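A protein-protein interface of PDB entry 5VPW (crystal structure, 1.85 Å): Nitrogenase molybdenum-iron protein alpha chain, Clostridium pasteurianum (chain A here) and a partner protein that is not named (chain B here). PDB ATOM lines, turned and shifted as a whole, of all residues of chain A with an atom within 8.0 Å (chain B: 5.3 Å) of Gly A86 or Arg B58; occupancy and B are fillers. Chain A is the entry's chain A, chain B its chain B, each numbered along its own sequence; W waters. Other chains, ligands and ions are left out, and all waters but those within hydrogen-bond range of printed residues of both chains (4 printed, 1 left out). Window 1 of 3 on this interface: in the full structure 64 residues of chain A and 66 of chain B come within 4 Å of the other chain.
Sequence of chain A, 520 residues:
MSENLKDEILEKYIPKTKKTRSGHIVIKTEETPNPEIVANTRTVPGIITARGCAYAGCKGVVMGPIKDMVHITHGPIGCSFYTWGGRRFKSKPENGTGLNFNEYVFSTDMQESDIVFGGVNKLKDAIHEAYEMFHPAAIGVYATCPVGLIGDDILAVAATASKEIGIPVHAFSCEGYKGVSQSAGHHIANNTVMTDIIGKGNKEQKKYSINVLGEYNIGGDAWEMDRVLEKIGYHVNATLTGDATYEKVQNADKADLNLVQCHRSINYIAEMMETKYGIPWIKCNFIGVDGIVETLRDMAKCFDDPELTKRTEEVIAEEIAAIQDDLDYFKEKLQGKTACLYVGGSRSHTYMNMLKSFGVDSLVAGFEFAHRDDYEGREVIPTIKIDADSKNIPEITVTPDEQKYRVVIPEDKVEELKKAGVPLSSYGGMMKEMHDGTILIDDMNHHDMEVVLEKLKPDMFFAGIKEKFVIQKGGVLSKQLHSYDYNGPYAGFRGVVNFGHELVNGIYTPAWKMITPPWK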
ATOM      1  N   GLY A  60      13.089 -23.713   4.987  1.00  0.00           N
ATOM      2  CA  GLY A  60      14.480 -23.472   5.263  1.00  0.00           C
ATOM      3  C   GLY A  60      14.741 -22.047   5.726  1.00  0.00           C
ATOM      4  O   GLY A  60      15.660 -21.806   6.512  1.00  0.00           O
ATOM      5  N   PHE A  81      17.314 -33.496   4.827  1.00  0.00           N
ATOM      6  CA  PHE A  81      18.782 -33.513   4.985  1.00  0.00           C
ATOM      7  C   PHE A  81      19.455 -32.209   4.591  1.00  0.00           C
ATOM      8  O   PHE A  81      20.419 -31.815   5.248  1.00  0.00           O
ATOM      9  CB  PHE A  81      19.378 -34.647   4.127  1.00  0.00           C
ATOM     10  CG  PHE A  81      20.873 -34.814   4.253  1.00  0.00           C
ATOM     11  CD1 PHE A  81      21.412 -35.660   5.201  1.00  0.00           C
ATOM     12  CD2 PHE A  81      21.735 -34.150   3.393  1.00  0.00           C
ATOM     13  CE1 PHE A  81      22.789 -35.807   5.322  1.00  0.00           C
ATOM     14  CE2 PHE A  81      23.098 -34.296   3.497  1.00  0.00           C
ATOM     15  CZ  PHE A  81      23.632 -35.108   4.467  1.00  0.00           C
ATOM     16  N   TYR A  82      19.014 -31.575   3.499  1.00  0.00           N
ATOM     17  CA  TYR A  82      19.666 -30.336   3.035  1.00  0.00           C
ATOM     18  C   TYR A  82      19.249 -29.061   3.772  1.00  0.00           C
ATOM     19  O   TYR A  82      19.690 -27.945   3.428  1.00  0.00           O
ATOM     20  CB  TYR A  82      19.478 -30.197   1.513  1.00  0.00           C
ATOM     21  CG  TYR A  82      20.194 -31.310   0.789  1.00  0.00           C
ATOM     22  CD1 TYR A  82      21.560 -31.440   0.903  1.00  0.00           C
ATOM     23  CD2 TYR A  82      19.489 -32.279   0.064  1.00  0.00           C
ATOM     24  CE1 TYR A  82      22.236 -32.482   0.282  1.00  0.00           C
ATOM     25  CE2 TYR A  82      20.146 -33.344  -0.545  1.00  0.00           C
ATOM     26  CZ  TYR A  82      21.514 -33.432  -0.446  1.00  0.00           C
ATOM     27  OH  TYR A  82      22.198 -34.434  -1.051  1.00  0.00           O
ATOM     28  N   THR A  83      18.378 -29.207   4.758  1.00  0.00           N
ATOM     29  CA  THR A  83      18.036 -28.123   5.665  1.00  0.00           C
ATOM     30  C   THR A  83      18.580 -28.438   7.057  1.00  0.00           C
ATOM     31  O   THR A  83      18.044 -27.974   8.039  1.00  0.00           O
ATOM     32  CB  THR A  83      16.505 -27.869   5.740  1.00  0.00           C
ATOM     33  OG1 THR A  83      15.760 -29.075   6.082  1.00  0.00           O
ATOM     34  CG2 THR A  83      16.012 -27.291   4.392  1.00  0.00           C
ATOM     35  N   TRP A  84      19.577 -29.309   7.143  1.00  0.00           N
ATOM     36  CA  TRP A  84      20.159 -29.687   8.451  1.00  0.00           C
ATOM     37  C   TRP A  84      21.419 -28.859   8.802  1.00  0.00           C
ATOM     38  O   TRP A  84      22.554 -29.326   8.647  1.00  0.00           O
ATOM     39  CB  TRP A  84      20.446 -31.181   8.418  1.00  0.00           C
ATOM     40  CG  TRP A  84      20.727 -31.841   9.711  1.00  0.00           C
ATOM     41  CD1 TRP A  84      20.685 -31.306  10.978  1.00  0.00           C
ATOM     42  CD2 TRP A  84      21.072 -33.217   9.874  1.00  0.00           C
ATOM     43  NE1 TRP A  84      21.007 -32.283  11.901  1.00  0.00           N
ATOM     44  CE2 TRP A  84      21.246 -33.453  11.246  1.00  0.00           C
ATOM     45  CE3 TRP A  84      21.238 -34.276   8.982  1.00  0.00           C
ATOM     46  CZ2 TRP A  84      21.614 -34.711  11.748  1.00  0.00           C
ATOM     47  CZ3 TRP A  84      21.626 -35.520   9.493  1.00  0.00           C
ATOM     48  CH2 TRP A  84      21.790 -35.716  10.844  1.00  0.00           C
ATOM     49  N   GLY A  85      21.188 -27.625   9.281  1.00  0.00           N
ATOM     50  CA  GLY A  85      22.239 -26.773   9.804  1.00  0.00           C
ATOM     51  C   GLY A  85      23.052 -25.931   8.832  1.00  0.00           C
ATOM     52  O   GLY A  85      23.926 -25.201   9.262  1.00  0.00           O
ATOM     53  N   GLY A  86      22.763 -26.020   7.529  1.00  0.00           N
ATOM     54  CA  GLY A  86      23.454 -25.227   6.527  1.00  0.00           C
ATOM     55  C   GLY A  86      23.181 -23.739   6.606  1.00  0.00           C
ATOM     56  O   GLY A  86      24.048 -22.948   6.263  1.00  0.00           O
ATOM     57  N   ARG A  87      21.974 -23.370   7.033  1.00  0.00           N
ATOM     58  CA  ARG A  87      21.630 -21.972   7.203  1.00  0.00           C
ATOM     59  C   ARG A  87      21.776 -21.669   8.708  1.00  0.00           C
ATOM     60  O   ARG A  87      21.147 -22.331   9.517  1.00  0.00           O
ATOM     61  CB  ARG A  87      20.207 -21.684   6.730  1.00  0.00           C
ATOM     62  CG  ARG A  87      19.857 -20.180   6.853  1.00  0.00           C
ATOM     63  CD  ARG A  87      18.688 -19.808   5.951  1.00  0.00           C
ATOM     64  NE  ARG A  87      18.124 -18.461   6.212  1.00  0.00           N
ATOM     65  CZ  ARG A  87      17.134 -18.209   7.062  1.00  0.00           C
ATOM     66  NH1 ARG A  87      16.661 -16.970   7.170  1.00  0.00           N
ATOM     67  NH2 ARG A  87      16.549 -19.190   7.733  1.00  0.00           N
ATOM     68  N   ARG A  88      22.558 -20.641   9.041  1.00  0.00           N
ATOM     69  CA  ARG A  88      23.122 -20.463  10.390  1.00  0.00           C
ATOM     70  C   ARG A  88      22.282 -19.561  11.324  1.00  0.00           C
ATOM     71  O   ARG A  88      22.811 -18.668  12.023  1.00  0.00           O
ATOM     72  CB  ARG A  88      24.559 -19.949  10.271  1.00  0.00           C
ATOM     73  CG  ARG A  88      25.490 -20.924   9.578  1.00  0.00           C
ATOM     74  CD  ARG A  88      26.911 -20.399   9.471  1.00  0.00           C
ATOM     75  NE  ARG A  88      27.457 -20.097  10.807  1.00  0.00           N
ATOM     76  CZ  ARG A  88      27.683 -18.884  11.282  1.00  0.00           C
ATOM     77  NH1 ARG A  88      28.113 -18.737  12.533  1.00  0.00           N
ATOM     78  NH2 ARG A  88      27.517 -17.821  10.511  1.00  0.00           N
ATOM     79  N   PHE A  89      20.971 -19.768  11.309  1.00  0.00           N
ATOM     80  CA  PHE A  89      20.104 -19.103  12.283  1.00  0.00           C
ATOM     81  C   PHE A  89      20.478 -19.623  13.663  1.00  0.00           C
ATOM     82  O   PHE A  89      20.613 -20.819  13.857  1.00  0.00           O
ATOM     83  CB  PHE A  89      18.598 -19.263  11.996  1.00  0.00           C
ATOM     84  CG  PHE A  89      18.142 -20.682  11.700  1.00  0.00           C
ATOM     85  CD1 PHE A  89      17.699 -21.491  12.704  1.00  0.00           C
ATOM     86  CD2 PHE A  89      18.054 -21.141  10.391  1.00  0.00           C
ATOM     87  CE1 PHE A  89      17.227 -22.776  12.427  1.00  0.00           C
ATOM     88  CE2 PHE A  89      17.617 -22.424  10.096  1.00  0.00           C
ATOM     89  CZ  PHE A  89      17.176 -23.243  11.124  1.00  0.00           C
ATOM     90  N   ASN A 102      16.939 -26.800  17.136  1.00  0.00           N
ATOM     91  CA  ASN A 102      17.855 -26.384  16.065  1.00  0.00           C
ATOM     92  C   ASN A 102      18.750 -27.525  15.571  1.00  0.00           C
ATOM     93  O   ASN A 102      19.200 -27.526  14.443  1.00  0.00           O
ATOM     94  CB  ASN A 102      18.763 -25.229  16.532  1.00  0.00           C
ATOM     95  CG  ASN A 102      18.326 -23.859  16.008  1.00  0.00           C
ATOM     96  OD1 ASN A 102      17.113 -23.502  15.962  1.00  0.00           O
ATOM     97  ND2 ASN A 102      19.332 -23.045  15.656  1.00  0.00           N
ATOM     98  N   VAL A 105      16.600 -32.448  12.365  1.00  0.00           N
ATOM     99  CA  VAL A 105      15.679 -32.304  11.226  1.00  0.00           C
ATOM    100  C   VAL A 105      14.712 -33.465  11.275  1.00  0.00           C
ATOM    101  O   VAL A 105      15.092 -34.590  11.635  1.00  0.00           O
ATOM    102  CB  VAL A 105      16.377 -32.263   9.849  1.00  0.00           C
ATOM    103  CG1 VAL A 105      17.045 -30.893   9.662  1.00  0.00           C
ATOM    104  CG2 VAL A 105      17.388 -33.383   9.704  1.00  0.00           C
ATOM    105  N   ILE A 218      21.071 -14.727  11.704  1.00  0.00           N
ATOM    106  CA  ILE A 218      22.165 -15.500  11.125  1.00  0.00           C
ATOM    107  C   ILE A 218      23.438 -15.086  11.850  1.00  0.00           C
ATOM    108  O   ILE A 218      23.780 -13.894  11.912  1.00  0.00           O
ATOM    109  CB  ILE A 218      22.295 -15.276   9.599  1.00  0.00           C
ATOM    110  CG1 ILE A 218      20.965 -15.541   8.914  1.00  0.00           C
ATOM    111  CG2 ILE A 218      23.453 -16.102   9.010  1.00  0.00           C
ATOM    112  CD1 ILE A 218      20.399 -16.931   9.122  1.00  0.00           C
ATOM    113  N   ILE A 465      28.079 -20.170  -1.329  1.00  0.00           N
ATOM    114  CA  ILE A 465      28.946 -21.359  -1.252  1.00  0.00           C
ATOM    115  C   ILE A 465      29.185 -22.008  -2.621  1.00  0.00           C
ATOM    116  O   ILE A 465      30.273 -22.535  -2.857  1.00  0.00           O
ATOM    117  CB  ILE A 465      28.415 -22.378  -0.203  1.00  0.00           C
ATOM    118  CG1 ILE A 465      29.453 -23.447   0.159  1.00  0.00           C
ATOM    119  CG2 ILE A 465      27.110 -23.010  -0.648  1.00  0.00           C
ATOM    120  CD1 ILE A 465      30.781 -22.921   0.652  1.00  0.00           C
ATOM    121  N   LYS A 466      28.210 -21.921  -3.526  1.00  0.00           N
ATOM    122  CA  LYS A 466      28.365 -22.530  -4.877  1.00  0.00           C
ATOM    123  C   LYS A 466      29.371 -21.783  -5.738  1.00  0.00           C
ATOM    124  O   LYS A 466      30.035 -22.364  -6.582  1.00  0.00           O
ATOM    125  CB  LYS A 466      27.011 -22.621  -5.573  1.00  0.00           C
ATOM    126  CG  LYS A 466      26.040 -23.552  -4.846  1.00  0.00           C
ATOM    127  CD  LYS A 466      24.746 -23.886  -5.575  1.00  0.00           C
ATOM    128  CE  LYS A 466      23.939 -22.677  -6.020  1.00  0.00           C
ATOM    129  NZ  LYS A 466      23.336 -21.930  -4.907  1.00  0.00           N
ATOM    130  N   PHE A 469      34.317 -20.994  -4.418  1.00  0.00           N
ATOM    131  CA  PHE A 469      35.535 -21.658  -4.838  1.00  0.00           C
ATOM    132  C   PHE A 469      35.770 -21.470  -6.325  1.00  0.00           C
ATOM    133  O   PHE A 469      36.926 -21.461  -6.791  1.00  0.00           O
ATOM    134  CB  PHE A 469      35.521 -23.155  -4.409  1.00  0.00           C
ATOM    135  CG  PHE A 469      35.431 -23.318  -2.904  1.00  0.00           C
ATOM    136  CD1 PHE A 469      36.443 -22.818  -2.094  1.00  0.00           C
ATOM    137  CD2 PHE A 469      34.295 -23.832  -2.311  1.00  0.00           C
ATOM    138  CE1 PHE A 469      36.346 -22.891  -0.730  1.00  0.00           C
ATOM    139  CE2 PHE A 469      34.207 -23.921  -0.941  1.00  0.00           C
ATOM    140  CZ  PHE A 469      35.239 -23.467  -0.152  1.00  0.00           C
ATOM    141  N   GLN A 480      31.680 -15.068   1.775  1.00  0.00           N
ATOM    142  CA  GLN A 480      30.286 -15.453   1.714  1.00  0.00           C
ATOM    143  C   GLN A 480      29.364 -14.469   2.411  1.00  0.00           C
ATOM    144  O   GLN A 480      29.551 -14.141   3.565  1.00  0.00           O
ATOM    145  CB  GLN A 480      30.087 -16.840   2.343  1.00  0.00           C
ATOM    146  CG  GLN A 480      30.793 -17.957   1.625  1.00  0.00           C
ATOM    147  CD  GLN A 480      30.475 -19.316   2.232  1.00  0.00           C
ATOM    148  OE1 GLN A 480      29.336 -19.824   2.150  1.00  0.00           O
ATOM    149  NE2 GLN A 480      31.486 -19.905   2.875  1.00  0.00           N
ATOM    150  N   HIS A 482      25.998 -15.137   2.712  1.00  0.00           N
ATOM    151  CA  HIS A 482      24.914 -15.828   3.350  1.00  0.00           C
ATOM    152  C   HIS A 482      25.385 -16.430   4.688  1.00  0.00           C
ATOM    153  O   HIS A 482      24.870 -16.065   5.753  1.00  0.00           O
ATOM    154  CB  HIS A 482      24.282 -16.960   2.534  1.00  0.00           C
ATOM    155  CG  HIS A 482      23.947 -16.636   1.108  1.00  0.00           C
ATOM    156  ND1 HIS A 482      22.664 -16.737   0.607  1.00  0.00           N
ATOM    157  CD2 HIS A 482      24.728 -16.296   0.061  1.00  0.00           C
ATOM    158  CE1 HIS A 482      22.681 -16.493  -0.688  1.00  0.00           C
ATOM    159  NE2 HIS A 482      23.917 -16.211  -1.043  1.00  0.00           N
ATOM    160  N   SER A 483      26.341 -17.366   4.628  1.00  0.00           N
ATOM    161  CA  SER A 483      26.874 -18.027   5.826  1.00  0.00           C
ATOM    162  C   SER A 483      27.878 -17.214   6.631  1.00  0.00           C
ATOM    163  O   SER A 483      28.272 -17.633   7.739  1.00  0.00           O
ATOM    164  CB  SER A 483      27.575 -19.335   5.409  1.00  0.00           C
ATOM    165  OG  SER A 483      28.770 -19.056   4.668  1.00  0.00           O
ATOM    166  N   TYR A 486      31.004 -18.780   8.425  1.00  0.00           N
ATOM    167  CA  TYR A 486      30.918 -19.497   9.692  1.00  0.00           C
ATOM    168  C   TYR A 486      31.341 -18.606  10.839  1.00  0.00           C
ATOM    169  O   TYR A 486      31.739 -19.112  11.884  1.00  0.00           O
ATOM    170  CB  TYR A 486      31.681 -20.874   9.603  1.00  0.00           C
ATOM    171  CG  TYR A 486      31.505 -21.422   8.205  1.00  0.00           C
ATOM    172  CD1 TYR A 486      30.258 -21.760   7.748  1.00  0.00           C
ATOM    173  CD2 TYR A 486      32.563 -21.469   7.303  1.00  0.00           C
ATOM    174  CE1 TYR A 486      30.059 -22.164   6.451  1.00  0.00           C
ATOM    175  CE2 TYR A 486      32.364 -21.877   5.985  1.00  0.00           C
ATOM    176  CZ  TYR A 486      31.095 -22.212   5.566  1.00  0.00           C
ATOM    177  OH  TYR A 486      30.826 -22.614   4.259  1.00  0.00           O
ATOM    178  N   ARG B  53      24.644 -29.449  -5.468  1.00  0.00           N
ATOM    179  CA  ARG B  53      25.922 -28.750  -5.702  1.00  0.00           C
ATOM    180  C   ARG B  53      26.485 -28.248  -4.374  1.00  0.00           C
ATOM    181  O   ARG B  53      27.686 -28.295  -4.119  1.00  0.00           O
ATOM    182  CB  ARG B  53      25.733 -27.556  -6.604  1.00  0.00           C
ATOM    183  CG  ARG B  53      25.377 -27.873  -8.055  1.00  0.00           C
ATOM    184  CD  ARG B  53      25.081 -26.598  -8.831  1.00  0.00           C
ATOM    185  NE  ARG B  53      26.299 -25.820  -8.986  1.00  0.00           N
ATOM    186  CZ  ARG B  53      26.349 -24.515  -9.240  1.00  0.00           C
ATOM    187  NH1 ARG B  53      25.247 -23.803  -9.401  1.00  0.00           N
ATOM    188  NH2 ARG B  53      27.532 -23.916  -9.297  1.00  0.00           N
ATOM    189  N   THR B  54      25.594 -27.770  -3.513  1.00  0.00           N
ATOM    190  CA  THR B  54      26.033 -27.162  -2.265  1.00  0.00           C
ATOM    191  C   THR B  54      26.758 -28.132  -1.337  1.00  0.00           C
ATOM    192  O   THR B  54      27.820 -27.834  -0.782  1.00  0.00           O
ATOM    193  CB  THR B  54      24.843 -26.477  -1.574  1.00  0.00           C
ATOM    194  OG1 THR B  54      24.486 -25.271  -2.303  1.00  0.00           O
ATOM    195  CG2 THR B  54      25.194 -26.125  -0.154  1.00  0.00           C
ATOM    196  N   VAL B  55      26.200 -29.321  -1.137  1.00  0.00           N
ATOM    197  CA  VAL B  55      26.826 -30.254  -0.234  1.00  0.00           C
ATOM    198  C   VAL B  55      28.180 -30.705  -0.752  1.00  0.00           C
ATOM    199  O   VAL B  55      29.107 -30.970   0.027  1.00  0.00           O
ATOM    200  CB  VAL B  55      25.924 -31.474   0.069  1.00  0.00           C
ATOM    201  CG1 VAL B  55      25.855 -32.397  -1.114  1.00  0.00           C
ATOM    202  CG2 VAL B  55      26.428 -32.226   1.304  1.00  0.00           C
ATOM    203  N   LEU B  56      28.321 -30.800  -2.070  1.00  0.00           N
ATOM    204  CA  LEU B  56      29.590 -31.205  -2.623  1.00  0.00           C
ATOM    205  C   LEU B  56      30.643 -30.118  -2.390  1.00  0.00           C
ATOM    206  O   LEU B  56      31.786 -30.425  -2.055  1.00  0.00           O
ATOM    207  CB  LEU B  56      29.476 -31.610  -4.108  1.00  0.00           C
ATOM    208  CG  LEU B  56      28.708 -32.892  -4.414  1.00  0.00           C
ATOM    209  CD1 LEU B  56      28.409 -32.964  -5.920  1.00  0.00           C
ATOM    210  CD2 LEU B  56      29.465 -34.116  -3.951  1.00  0.00           C
ATOM    211  N   SER B  57      30.283 -28.848  -2.526  1.00  0.00           N
ATOM    212  CA  SER B  57      31.216 -27.791  -2.209  1.00  0.00           C
ATOM    213  C   SER B  57      31.550 -27.715  -0.709  1.00  0.00           C
ATOM    214  O   SER B  57      32.721 -27.484  -0.335  1.00  0.00           O
ATOM    215  CB  SER B  57      30.712 -26.410  -2.729  1.00  0.00           C
ATOM    216  OG  SER B  57      30.814 -26.299  -4.155  1.00  0.00           O
ATOM    217  N   ARG B  58      30.568 -27.920   0.158  1.00  0.00           N
ATOM    218  CA  ARG B  58      30.852 -27.945   1.600  1.00  0.00           C
ATOM    219  C   ARG B  58      31.801 -29.086   2.008  1.00  0.00           C
ATOM    220  O   ARG B  58      32.628 -28.925   2.923  1.00  0.00           O
ATOM    221  CB  ARG B  58      29.584 -28.013   2.399  1.00  0.00           C
ATOM    222  CG  ARG B  58      28.728 -26.749   2.315  1.00  0.00           C
ATOM    223  CD  ARG B  58      27.361 -26.928   2.949  1.00  0.00           C
ATOM    224  NE  ARG B  58      26.668 -25.656   3.000  1.00  0.00           N
ATOM    225  CZ  ARG B  58      25.353 -25.500   3.119  1.00  0.00           C
ATOM    226  NH1 ARG B  58      24.519 -26.559   3.233  1.00  0.00           N
ATOM    227  NH2 ARG B  58      24.870 -24.251   3.122  1.00  0.00           N
ATOM    228  N   HIS B  59      31.639 -30.241   1.391  1.00  0.00           N
ATOM    229  CA  HIS B  59      32.508 -31.406   1.651  1.00  0.00           C
ATOM    230  C   HIS B  59      33.911 -31.251   1.063  1.00  0.00           C
ATOM    231  O   HIS B  59      34.899 -31.420   1.779  1.00  0.00           O
ATOM    232  CB  HIS B  59      31.846 -32.698   1.133  1.00  0.00           C
ATOM    233  CG  HIS B  59      32.697 -33.929   1.261  1.00  0.00           C
ATOM    234  ND1 HIS B  59      32.564 -34.822   2.306  1.00  0.00           N
ATOM    235  CD2 HIS B  59      33.701 -34.407   0.487  1.00  0.00           C
ATOM    236  CE1 HIS B  59      33.447 -35.799   2.168  1.00  0.00           C
ATOM    237  NE2 HIS B  59      34.133 -35.585   1.059  1.00  0.00           N
ATOM    238  N   PHE B  60      34.003 -30.896  -0.227  1.00  0.00           N
ATOM    239  CA  PHE B  60      35.277 -30.865  -0.914  1.00  0.00           C
ATOM    240  C   PHE B  60      36.021 -29.514  -0.855  1.00  0.00           C
ATOM    241  O   PHE B  60      37.247 -29.454  -1.155  1.00  0.00           O
ATOM    242  CB  PHE B  60      35.065 -31.304  -2.386  1.00  0.00           C
ATOM    243  CG  PHE B  60      34.802 -32.751  -2.522  1.00  0.00           C
ATOM    244  CD1 PHE B  60      35.819 -33.650  -2.250  1.00  0.00           C
ATOM    245  CD2 PHE B  60      33.556 -33.222  -2.861  1.00  0.00           C
ATOM    246  CE1 PHE B  60      35.579 -34.999  -2.330  1.00  0.00           C
ATOM    247  CE2 PHE B  60      33.321 -34.566  -2.969  1.00  0.00           C
ATOM    248  CZ  PHE B  60      34.333 -35.456  -2.681  1.00  0.00           C
ATOM    249  N   LYS B  61      35.311 -28.449  -0.466  1.00  0.00           N
ATOM    250  CA  LYS B  61      35.858 -27.079  -0.538  1.00  0.00           C
ATOM    251  C   LYS B  61      36.389 -26.814  -1.967  1.00  0.00           C
ATOM    252  O   LYS B  61      37.502 -26.318  -2.159  1.00  0.00           O
ATOM    253  CB  LYS B  61      36.968 -26.889   0.498  1.00  0.00           C
ATOM    254  CG  LYS B  61      36.617 -27.300   1.939  1.00  0.00           C
ATOM    255  CD  LYS B  61      35.359 -26.682   2.507  1.00  0.00           C
ATOM    256  CE  LYS B  61      35.153 -27.046   3.979  1.00  0.00           C
ATOM    257  NZ  LYS B  61      33.742 -26.761   4.433  1.00  0.00           N
ATOM    258  N   ILE B 413      31.708 -34.659   5.158  1.00  0.00           N
ATOM    259  CA  ILE B 413      32.546 -34.080   6.157  1.00  0.00           C
ATOM    260  C   ILE B 413      32.721 -32.627   5.738  1.00  0.00           C
ATOM    261  O   ILE B 413      33.393 -32.356   4.766  1.00  0.00           O
ATOM    262  CB  ILE B 413      33.927 -34.758   6.233  1.00  0.00           C
ATOM    263  CG1 ILE B 413      33.752 -36.241   6.604  1.00  0.00           C
ATOM    264  CG2 ILE B 413      34.804 -34.064   7.290  1.00  0.00           C
ATOM    265  CD1 ILE B 413      35.041 -37.029   6.541  1.00  0.00           C
ATOM    266  N   MET B 414      32.115 -31.722   6.482  1.00  0.00           N
ATOM    267  CA  MET B 414      31.990 -30.310   6.055  1.00  0.00           C
ATOM    268  C   MET B 414      32.705 -29.360   6.982  1.00  0.00           C
ATOM    269  O   MET B 414      32.640 -28.152   6.780  1.00  0.00           O
ATOM    270  CB  MET B 414      30.523 -29.958   5.982  1.00  0.00           C
ATOM    271  CG  MET B 414      29.772 -30.844   4.979  1.00  0.00           C
ATOM    272  SD  MET B 414      28.041 -30.503   4.766  1.00  0.00           S
ATOM    273  CE  MET B 414      27.448 -30.950   6.384  1.00  0.00           C
ATOM    274  N   ASP B 415      33.413 -29.892   7.969  1.00  0.00           N
ATOM    275  CA  ASP B 415      33.928 -29.081   9.055  1.00  0.00           C
ATOM    276  C   ASP B 415      35.430 -29.221   9.408  1.00  0.00           C
ATOM    277  O   ASP B 415      35.871 -28.726  10.422  1.00  0.00           O
ATOM    278  CB  ASP B 415      33.048 -29.238  10.312  1.00  0.00           C
ATOM    279  CG  ASP B 415      33.044 -30.639  10.872  1.00  0.00           C
ATOM    280  OD1 ASP B 415      33.364 -31.551  10.125  1.00  0.00           O
ATOM    281  OD2 ASP B 415      32.683 -30.833  12.073  1.00  0.00           O
HETATM  282  O   HOH W   1      28.102 -23.151   3.754  1.00  0.00           O
HETATM  283  O   HOH W   2      21.808 -26.918   2.042  1.00  0.00           O
HETATM  284  O   HOH W   3      32.911 -24.286   3.264  1.00  0.00           O
HETATM  285  O   HOH W   4      23.144 -22.962  -2.155  1.00  0.00           O
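Hydrophobic or aromatic side chains of chain A that line the printed part of chain B: Tyr A82, Ile A465 and Phe A469.
Of the 12 printed residues of chain B, 6 touch a printed residue of chain A.
Among the printed residues, 8 pairs touch across the chains.
Water W4 bridges the side-chain hydroxyl (OG1) of Thr B54 (2.7 Å) and the side-chain amino group (NZ) of Lys A466 (2.9 Å).
Water W2 lies within hydrogen-bond range of the backbone carbonyl oxygen of Tyr A82 and the guanidinium group of Arg B58.
Water W1 lies within hydrogen-bond range of OH of Tyr A486 (2.8 Å) and NE of Arg B58 (3.0 Å).
Water W3 bridges OH of Tyr A486 and NZ of Lys B61.
O of Gly A86 sits at hydrogen-bond distance from NH2 of Arg B58 (3.5 Å).
The side-chain amino group of Lys B61 lies within hydrogen-bond range of the backbone carbonyl oxygen of Arg B58, at 2.9 Å.
NZ of Lys B61 lies within hydrogen-bond range of O of Met B414, at 2.9 Å.
Among the printed residues, pairs that only touch across the chains: Tyr A82 with Val B55, Ile A465 with Thr B54, Ile A465 with Ser B57, Lys A466 with Arg B53, Lys A466 with Thr B54, Phe A469 with Ser B57 and Phe A469 with Lys B61.
Of the printed residues of chain B, Tyr A82 touches Val B55.
Gly A86 touches just one residue of chain B: Arg B58.
Printed residues of chain B within 4 Å of Ile A465: Thr B54 and Ser B57.
Printed residues of chain A within 4 Å of Ser B57: Ile A465 and Phe A469.
Of the printed residues of chain A, Arg B58 touches Gly A86.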
